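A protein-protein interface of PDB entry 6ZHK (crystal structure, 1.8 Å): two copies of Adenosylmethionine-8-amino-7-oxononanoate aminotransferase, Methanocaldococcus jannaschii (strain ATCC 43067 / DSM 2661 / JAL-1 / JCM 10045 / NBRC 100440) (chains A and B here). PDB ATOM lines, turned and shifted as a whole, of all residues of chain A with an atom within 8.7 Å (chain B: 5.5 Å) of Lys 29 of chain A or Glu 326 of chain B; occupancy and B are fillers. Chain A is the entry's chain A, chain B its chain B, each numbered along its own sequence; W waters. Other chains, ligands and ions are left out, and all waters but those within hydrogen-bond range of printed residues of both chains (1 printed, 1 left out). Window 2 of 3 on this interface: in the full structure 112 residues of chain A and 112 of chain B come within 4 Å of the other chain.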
ATOM      1  N   LYS A  18      30.077  24.987 -31.012  1.00  0.00           N
ATOM      2  CA  LYS A  18      30.808  24.396 -29.906  1.00  0.00           C
ATOM      3  C   LYS A  18      32.286  24.723 -30.041  1.00  0.00           C
ATOM      4  O   LYS A  18      33.006  24.725 -29.063  1.00  0.00           O
ATOM      5  CB  LYS A  18      30.557  22.873 -29.915  1.00  0.00           C
ATOM      6  CG  LYS A  18      29.156  22.465 -29.453  1.00  0.00           C
ATOM      7  CD  LYS A  18      28.778  21.003 -29.854  1.00  0.00           C
ATOM      8  CE  LYS A  18      27.385  20.673 -29.353  1.00  0.00           C
ATOM      9  NZ  LYS A  18      27.055  19.214 -29.435  1.00  0.00           N
ATOM     10  N   TRP A  22      32.685  30.900 -26.898  1.00  0.00           N
ATOM     11  CA  TRP A  22      32.635  30.750 -25.449  1.00  0.00           C
ATOM     12  C   TRP A  22      31.322  31.373 -24.982  1.00  0.00           C
ATOM     13  O   TRP A  22      31.184  32.608 -24.982  1.00  0.00           O
ATOM     14  CB  TRP A  22      33.874  31.438 -24.853  1.00  0.00           C
ATOM     15  CG  TRP A  22      34.150  31.163 -23.402  1.00  0.00           C
ATOM     16  CD1 TRP A  22      33.266  30.783 -22.426  1.00  0.00           C
ATOM     17  CD2 TRP A  22      35.392  31.395 -22.738  1.00  0.00           C
ATOM     18  NE1 TRP A  22      33.918  30.673 -21.219  1.00  0.00           N
ATOM     19  CE2 TRP A  22      35.219  31.032 -21.378  1.00  0.00           C
ATOM     20  CE3 TRP A  22      36.651  31.802 -23.171  1.00  0.00           C
ATOM     21  CZ2 TRP A  22      36.242  31.132 -20.441  1.00  0.00           C
ATOM     22  CZ3 TRP A  22      37.672  31.891 -22.241  1.00  0.00           C
ATOM     23  CH2 TRP A  22      37.482  31.504 -20.912  1.00  0.00           C
ATOM     24  N   THR A  26      27.885  29.428 -19.024  1.00  0.00           N
ATOM     25  CA  THR A  26      27.673  28.087 -19.524  1.00  0.00           C
ATOM     26  C   THR A  26      28.948  27.264 -19.314  1.00  0.00           C
ATOM     27  O   THR A  26      30.045  27.679 -19.710  1.00  0.00           O
ATOM     28  CB  THR A  26      27.415  28.143 -21.053  1.00  0.00           C
ATOM     29  OG1 THR A  26      26.171  28.769 -21.425  1.00  0.00           O
ATOM     30  CG2 THR A  26      27.449  26.761 -21.703  1.00  0.00           C
ATOM     31  N   GLN A  27      28.790  26.064 -18.739  1.00  0.00           N
ATOM     32  CA  GLN A  27      29.922  25.162 -18.605  1.00  0.00           C
ATOM     33  C   GLN A  27      30.116  24.513 -19.966  1.00  0.00           C
ATOM     34  O   GLN A  27      29.349  23.618 -20.332  1.00  0.00           O
ATOM     35  CB  GLN A  27      29.651  24.131 -17.487  1.00  0.00           C
ATOM     36  CG  GLN A  27      30.650  23.000 -17.442  1.00  0.00           C
ATOM     37  CD  GLN A  27      32.086  23.450 -17.563  1.00  0.00           C
ATOM     38  OE1 GLN A  27      32.686  23.262 -18.609  1.00  0.00           O
ATOM     39  NE2 GLN A  27      32.632  24.078 -16.519  1.00  0.00           N
ATOM     40  N   MET A  28      31.179  24.909 -20.684  1.00  0.00           N
ATOM     41  CA  MET A  28      31.310  24.592 -22.097  1.00  0.00           C
ATOM     42  C   MET A  28      31.573  23.086 -22.277  1.00  0.00           C
ATOM     43  O   MET A  28      31.263  22.535 -23.327  1.00  0.00           O
ATOM     44  CB  MET A  28      32.455  25.401 -22.704  1.00  0.00           C
ATOM     45  CG  MET A  28      32.065  26.916 -22.972  1.00  0.00           C
ATOM     46  SD  MET A  28      30.473  27.086 -23.892  1.00  0.00           S
ATOM     47  CE  MET A  28      31.055  26.431 -25.459  1.00  0.00           C
ATOM     48  N   LYS A  29      32.166  22.448 -21.275  1.00  0.00           N
ATOM     49  CA  LYS A  29      32.327  20.986 -21.310  1.00  0.00           C
ATOM     50  C   LYS A  29      30.981  20.332 -21.559  1.00  0.00           C
ATOM     51  O   LYS A  29      30.871  19.440 -22.385  1.00  0.00           O
ATOM     52  CB  LYS A  29      33.064  20.456 -20.077  1.00  0.00           C
ATOM     53  CG  LYS A  29      33.020  18.931 -19.916  1.00  0.00           C
ATOM     54  CD  LYS A  29      34.233  18.289 -19.291  1.00  0.00           C
ATOM     55  CE  LYS A  29      34.125  16.764 -19.322  1.00  0.00           C
ATOM     56  NZ  LYS A  29      32.740  16.324 -18.969  1.00  0.00           N
ATOM     57  N   GLU A  30      29.958  20.746 -20.809  1.00  0.00           N
ATOM     58  CA  GLU A  30      28.662  20.110 -20.890  1.00  0.00           C
ATOM     59  C   GLU A  30      27.912  20.547 -22.131  1.00  0.00           C
ATOM     60  O   GLU A  30      27.219  19.745 -22.738  1.00  0.00           O
ATOM     61  CB  GLU A  30      27.862  20.386 -19.624  1.00  0.00           C
ATOM     62  CG  GLU A  30      28.517  19.565 -18.548  1.00  0.00           C
ATOM     63  CD  GLU A  30      27.695  19.429 -17.293  1.00  0.00           C
ATOM     64  OE1 GLU A  30      26.558  19.995 -17.263  1.00  0.00           O
ATOM     65  OE2 GLU A  30      28.205  18.752 -16.363  1.00  0.00           O
ATOM     66  N   TYR A  31      28.045  21.819 -22.488  1.00  0.00           N
ATOM     67  CA  TYR A  31      27.379  22.322 -23.671  1.00  0.00           C
ATOM     68  C   TYR A  31      27.893  21.560 -24.901  1.00  0.00           C
ATOM     69  O   TYR A  31      27.139  21.212 -25.802  1.00  0.00           O
ATOM     70  CB  TYR A  31      27.655  23.845 -23.727  1.00  0.00           C
ATOM     71  CG  TYR A  31      26.909  24.563 -24.826  1.00  0.00           C
ATOM     72  CD1 TYR A  31      25.623  25.034 -24.617  1.00  0.00           C
ATOM     73  CD2 TYR A  31      27.503  24.792 -26.067  1.00  0.00           C
ATOM     74  CE1 TYR A  31      24.929  25.714 -25.609  1.00  0.00           C
ATOM     75  CE2 TYR A  31      26.788  25.403 -27.093  1.00  0.00           C
ATOM     76  CZ  TYR A  31      25.510  25.895 -26.850  1.00  0.00           C
ATOM     77  OH  TYR A  31      24.797  26.494 -27.863  1.00  0.00           O
ATOM     78  N   ARG A  32      29.196  21.294 -24.940  1.00  0.00           N
ATOM     79  CA  ARG A  32      29.756  20.609 -26.089  1.00  0.00           C
ATOM     80  C   ARG A  32      29.286  19.157 -26.195  1.00  0.00           C
ATOM     81  O   ARG A  32      29.368  18.589 -27.282  1.00  0.00           O
ATOM     82  CB  ARG A  32      31.275  20.584 -26.038  1.00  0.00           C
ATOM     83  CG  ARG A  32      31.870  21.919 -26.446  1.00  0.00           C
ATOM     84  CD  ARG A  32      33.219  21.903 -25.765  1.00  0.00           C
ATOM     85  NE  ARG A  32      33.971  22.710 -26.704  1.00  0.00           N
ATOM     86  CZ  ARG A  32      35.280  22.881 -26.691  1.00  0.00           C
ATOM     87  NH1 ARG A  32      36.036  22.227 -25.816  1.00  0.00           N
ATOM     88  NH2 ARG A  32      35.805  23.678 -27.597  1.00  0.00           N
ATOM     89  N   GLU A  33      28.779  18.591 -25.094  1.00  0.00           N
ATOM     90  CA  GLU A  33      28.310  17.211 -25.125  1.00  0.00           C
ATOM     91  C   GLU A  33      26.849  17.142 -25.539  1.00  0.00           C
ATOM     92  O   GLU A  33      26.397  16.083 -25.941  1.00  0.00           O
ATOM     93  CB  GLU A  33      28.480  16.521 -23.781  1.00  0.00           C
ATOM     94  CG  GLU A  33      29.904  16.072 -23.574  1.00  0.00           C
ATOM     95  CD  GLU A  33      30.261  15.809 -22.122  1.00  0.00           C
ATOM     96  OE1 GLU A  33      29.400  16.048 -21.206  1.00  0.00           O
ATOM     97  OE2 GLU A  33      31.405  15.375 -21.899  1.00  0.00           O
ATOM     98  N   SER A  34      26.095  18.241 -25.388  1.00  0.00           N
ATOM     99  CA  SER A  34      24.656  18.120 -25.552  1.00  0.00           C
ATOM    100  C   SER A  34      24.181  18.596 -26.929  1.00  0.00           C
ATOM    101  O   SER A  34      24.941  19.170 -27.729  1.00  0.00           O
ATOM    102  CB  SER A  34      23.900  18.767 -24.406  1.00  0.00           C
ATOM    103  OG  SER A  34      24.391  20.089 -24.183  1.00  0.00           O
ATOM    104  N   ASN A  36      21.960  21.288 -28.451  1.00  0.00           N
ATOM    105  CA  ASN A  36      21.546  22.584 -27.935  1.00  0.00           C
ATOM    106  C   ASN A  36      20.635  23.267 -28.940  1.00  0.00           C
ATOM    107  O   ASN A  36      20.759  23.073 -30.135  1.00  0.00           O
ATOM    108  CB  ASN A  36      22.763  23.495 -27.653  1.00  0.00           C
ATOM    109  CG  ASN A  36      23.784  22.781 -26.788  1.00  0.00           C
ATOM    110  OD1 ASN A  36      23.433  22.343 -25.705  1.00  0.00           O
ATOM    111  ND2 ASN A  36      24.994  22.559 -27.275  1.00  0.00           N
ATOM    112  N   TYR A 411      23.879  21.385  -5.939  1.00  0.00           N
ATOM    113  CA  TYR A 411      24.073  22.197  -7.139  1.00  0.00           C
ATOM    114  C   TYR A 411      24.279  21.290  -8.352  1.00  0.00           C
ATOM    115  O   TYR A 411      23.701  21.521  -9.419  1.00  0.00           O
ATOM    116  CB  TYR A 411      25.281  23.128  -6.985  1.00  0.00           C
ATOM    117  CG  TYR A 411      25.452  24.137  -8.094  1.00  0.00           C
ATOM    118  CD1 TYR A 411      24.478  25.081  -8.376  1.00  0.00           C
ATOM    119  CD2 TYR A 411      26.614  24.164  -8.862  1.00  0.00           C
ATOM    120  CE1 TYR A 411      24.633  26.002  -9.419  1.00  0.00           C
ATOM    121  CE2 TYR A 411      26.799  25.098  -9.878  1.00  0.00           C
ATOM    122  CZ  TYR A 411      25.808  26.022 -10.148  1.00  0.00           C
ATOM    123  OH  TYR A 411      25.965  26.956 -11.130  1.00  0.00           O
ATOM    124  N   GLY A 412      25.110  20.257  -8.179  1.00  0.00           N
ATOM    125  CA  GLY A 412      25.571  19.448  -9.295  1.00  0.00           C
ATOM    126  C   GLY A 412      24.452  18.617  -9.911  1.00  0.00           C
ATOM    127  O   GLY A 412      24.609  18.093 -11.002  1.00  0.00           O
ATOM    128  N   LYS A 414      21.483  19.699 -10.890  1.00  0.00           N
ATOM    129  CA  LYS A 414      20.819  20.416 -11.985  1.00  0.00           C
ATOM    130  C   LYS A 414      19.325  20.106 -12.013  1.00  0.00           C
ATOM    131  O   LYS A 414      18.758  19.803 -13.073  1.00  0.00           O
ATOM    132  CB  LYS A 414      21.476  20.072 -13.332  1.00  0.00           C
ATOM    133  CG  LYS A 414      22.955  20.474 -13.415  1.00  0.00           C
ATOM    134  CD  LYS A 414      23.666  20.105 -14.725  1.00  0.00           C
ATOM    135  CE  LYS A 414      23.277  20.955 -15.920  1.00  0.00           C
ATOM    136  NZ  LYS A 414      23.753  20.375 -17.205  1.00  0.00           N
ATOM    137  N   LEU B 324      36.786  24.539 -18.148  1.00  0.00           N
ATOM    138  CA  LEU B 324      36.098  23.273 -18.413  1.00  0.00           C
ATOM    139  C   LEU B 324      36.011  22.372 -17.184  1.00  0.00           C
ATOM    140  O   LEU B 324      36.980  22.256 -16.436  1.00  0.00           O
ATOM    141  CB  LEU B 324      36.915  22.547 -19.494  1.00  0.00           C
ATOM    142  CG  LEU B 324      36.897  23.231 -20.855  1.00  0.00           C
ATOM    143  CD1 LEU B 324      37.795  22.497 -21.857  1.00  0.00           C
ATOM    144  CD2 LEU B 324      35.471  23.351 -21.384  1.00  0.00           C
ATOM    145  N   GLY B 325      34.826  21.778 -16.980  1.00  0.00           N
ATOM    146  CA  GLY B 325      34.661  20.703 -16.009  1.00  0.00           C
ATOM    147  C   GLY B 325      33.193  20.350 -15.830  1.00  0.00           C
ATOM    148  O   GLY B 325      32.356  20.730 -16.647  1.00  0.00           O
ATOM    149  N   GLU B 326      32.880  19.588 -14.766  1.00  0.00           N
ATOM    150  CA  GLU B 326      31.495  19.199 -14.548  1.00  0.00           C
ATOM    151  C   GLU B 326      30.758  20.414 -14.007  1.00  0.00           C
ATOM    152  O   GLU B 326      31.342  21.239 -13.330  1.00  0.00           O
ATOM    153  CB  GLU B 326      31.337  18.066 -13.524  1.00  0.00           C
ATOM    154  CG  GLU B 326      32.497  17.109 -13.446  1.00  0.00           C
ATOM    155  CD  GLU B 326      32.134  15.885 -14.249  1.00  0.00           C
ATOM    156  OE1 GLU B 326      31.442  14.997 -13.685  1.00  0.00           O
ATOM    157  OE2 GLU B 326      32.502  15.855 -15.443  1.00  0.00           O
ATOM    158  N   PHE B 327      29.468  20.507 -14.302  1.00  0.00           N
ATOM    159  CA  PHE B 327      28.698  21.647 -13.845  1.00  0.00           C
ATOM    160  C   PHE B 327      28.927  21.936 -12.357  1.00  0.00           C
ATOM    161  O   PHE B 327      29.074  23.088 -11.957  1.00  0.00           O
ATOM    162  CB  PHE B 327      27.227  21.356 -14.081  1.00  0.00           C
ATOM    163  CG  PHE B 327      26.350  22.546 -13.786  1.00  0.00           C
ATOM    164  CD1 PHE B 327      26.176  23.535 -14.745  1.00  0.00           C
ATOM    165  CD2 PHE B 327      25.731  22.670 -12.557  1.00  0.00           C
ATOM    166  CE1 PHE B 327      25.342  24.609 -14.474  1.00  0.00           C
ATOM    167  CE2 PHE B 327      24.919  23.749 -12.277  1.00  0.00           C
ATOM    168  CZ  PHE B 327      24.749  24.734 -13.232  1.00  0.00           C
ATOM    169  N   GLY B 328      28.903  20.890 -11.517  1.00  0.00           N
ATOM    170  CA  GLY B 328      28.863  21.085 -10.073  1.00  0.00           C
ATOM    171  C   GLY B 328      30.227  21.498  -9.513  1.00  0.00           C
ATOM    172  O   GLY B 328      30.351  21.855  -8.352  1.00  0.00           O
ATOM    173  N   GLU B 329      31.253  21.484 -10.360  1.00  0.00           N
ATOM    174  CA  GLU B 329      32.550  22.024  -9.977  1.00  0.00           C
ATOM    175  C   GLU B 329      32.542  23.554 -10.034  1.00  0.00           C
ATOM    176  O   GLU B 329      33.436  24.176  -9.497  1.00  0.00           O
ATOM    177  CB  GLU B 329      33.626  21.515 -10.940  1.00  0.00           C
ATOM    178  CG  GLU B 329      33.825  20.000 -10.873  1.00  0.00           C
ATOM    179  CD  GLU B 329      35.042  19.632 -11.709  1.00  0.00           C
ATOM    180  OE1 GLU B 329      36.136  19.679 -11.178  1.00  0.00           O
ATOM    181  OE2 GLU B 329      34.897  19.419 -12.917  1.00  0.00           O
ATOM    182  N   SER B 330      31.526  24.163 -10.663  1.00  0.00           N
ATOM    183  CA  SER B 330      31.398  25.614 -10.657  1.00  0.00           C
ATOM    184  C   SER B 330      32.656  26.361 -11.153  1.00  0.00           C
ATOM    185  O   SER B 330      33.099  27.358 -10.578  1.00  0.00           O
ATOM    186  CB  SER B 330      30.892  26.053  -9.292  1.00  0.00           C
ATOM    187  OG  SER B 330      30.455  27.364  -9.385  1.00  0.00           O
ATOM    188  N   LYS B 331      33.244  25.880 -12.254  1.00  0.00           N
ATOM    189  CA  LYS B 331      34.415  26.457 -12.896  1.00  0.00           C
ATOM    190  C   LYS B 331      34.058  27.323 -14.119  1.00  0.00           C
ATOM    191  O   LYS B 331      34.959  27.904 -14.721  1.00  0.00           O
ATOM    192  CB  LYS B 331      35.303  25.324 -13.413  1.00  0.00           C
ATOM    193  CG  LYS B 331      35.920  24.517 -12.278  1.00  0.00           C
ATOM    194  CD  LYS B 331      36.658  23.313 -12.704  1.00  0.00           C
ATOM    195  CE  LYS B 331      37.869  23.696 -13.496  1.00  0.00           C
ATOM    196  NZ  LYS B 331      38.402  22.522 -14.229  1.00  0.00           N
ATOM    197  N   GLN B 332      32.784  27.389 -14.507  1.00  0.00           N
ATOM    198  CA  GLN B 332      32.406  28.144 -15.705  1.00  0.00           C
ATOM    199  C   GLN B 332      32.572  29.638 -15.402  1.00  0.00           C
ATOM    200  O   GLN B 332      32.578  30.023 -14.222  1.00  0.00           O
ATOM    201  CB  GLN B 332      30.973  27.823 -16.181  1.00  0.00           C
ATOM    202  CG  GLN B 332      29.813  28.161 -15.219  1.00  0.00           C
ATOM    203  CD  GLN B 332      29.463  26.965 -14.340  1.00  0.00           C
ATOM    204  OE1 GLN B 332      30.327  26.383 -13.663  1.00  0.00           O
ATOM    205  NE2 GLN B 332      28.200  26.574 -14.350  1.00  0.00           N
HETATM  206  O   HOH W   1      27.429  18.260 -11.794  1.00  0.00           O
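No position is printed for both chains.
The side-chain amide oxygen of Gln 27 of chain A is in hydrogen-bond range of the backbone NH of Lys 29 of chain A.
The side-chain amino group (NZ) of Lys 29 of chain A is in salt-bridge range of the side-chain carboxylate (OE2) of Glu 33 of chain A (3.4 Å).
The backbone carbonyl oxygen of Glu 30 of chain A lies within hydrogen-bond range of the side-chain hydroxyl of Ser 34 of chain A.
NZ of Lys 414 of chain A lies within salt-bridge range of OE1 of Glu 30 of chain A, 2.8 Å away.
The backbone carbonyl oxygen (O) of Leu 324 of chain B lies within hydrogen-bond range of the side-chain amino group (NZ) of Lys 331 of chain B.
The backbone NH (N) of Glu 326 of chain B is in hydrogen-bond range of the side-chain carboxylate (OE2) of Glu 329 of chain B.
Water W1 lies within hydrogen-bond range of O of Gly 412 of chain A and N of Gly 328 of chain B.
The backbone NH (N) of Gly 325 of chain B is in hydrogen-bond range of the side-chain amide oxygen (OE1) of Gln 27 of chain A (3.1 Å).
OE2 of Glu 326 of chain B lies within salt-bridge range of NZ of Lys 29 of chain A, 3.6 Å away.
The side-chain carboxylate (OE2) of Glu 30 of chain A is in hydrogen-bond range of the backbone NH (N) of Phe 327 of chain B (3.0 Å).
Of the 9 printed residues of chain B, 6 touch a printed residue of chain A.
Hydrophobic or aromatic side chains of chain B that line the printed part of chain A: Leu 324 and Phe 327.
Along chain B the printed residues that touch a printed residue of chain A span positions 324 to 332.
Among the printed residues, 14 pairs touch across the chains.
CB of Gln 332 of chain B touches O of Thr 26 of chain A, at 3.7 Å.
Gln 27 of chain A touches Leu 324 of chain B (OE1 to CA, 3.4 Å).
Gln 27 of chain A touches Gln 332 of chain B.
CD2 of Leu 324 of chain B touches CB of Met 28 of chain A, 3.9 Å away.
Lys 29 of chain A touches Leu 324 of chain B (N to CD2, 3.4 Å).
Gly 325 of chain B touches Lys 29 of chain A (O to CB, 3.5 Å).
CA of Glu 326 of chain B touches OE2 of Glu 30 of chain A, at 3.8 Å.
Tyr 411 of chain A touches Phe 327 of chain B.
Gln 332 of chain B touches Tyr 411 of chain A.
CD2 of Phe 327 of chain B touches CG of Lys 414 of chain A, 3.6 Å away.
Of the printed residues of chain B, Gln 27 of chain A touches Leu 324 (3.4 Å), Gly 325 (2.9 Å) and Gln 332 (3.7 Å).
Of the printed residues of chain B, Gly 412 of chain A touches Gly 328 (3.8 Å).
Gly 325 of chain B touches two residues of chain A.
Printed residues of chain A within 4 Å of Glu 326 of chain B: Lys 29 and Glu 30.
Lys 331 of chain B touches none of the printed residues of chain A.
The nearest residue of chain A that does not touch Glu 326 of chain B is Gln 27 of chain A (4.3 Å).
The nearest printed residue of chain A that does not touch Gln 332 of chain B is Met 28 of chain A (5.4 Å).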
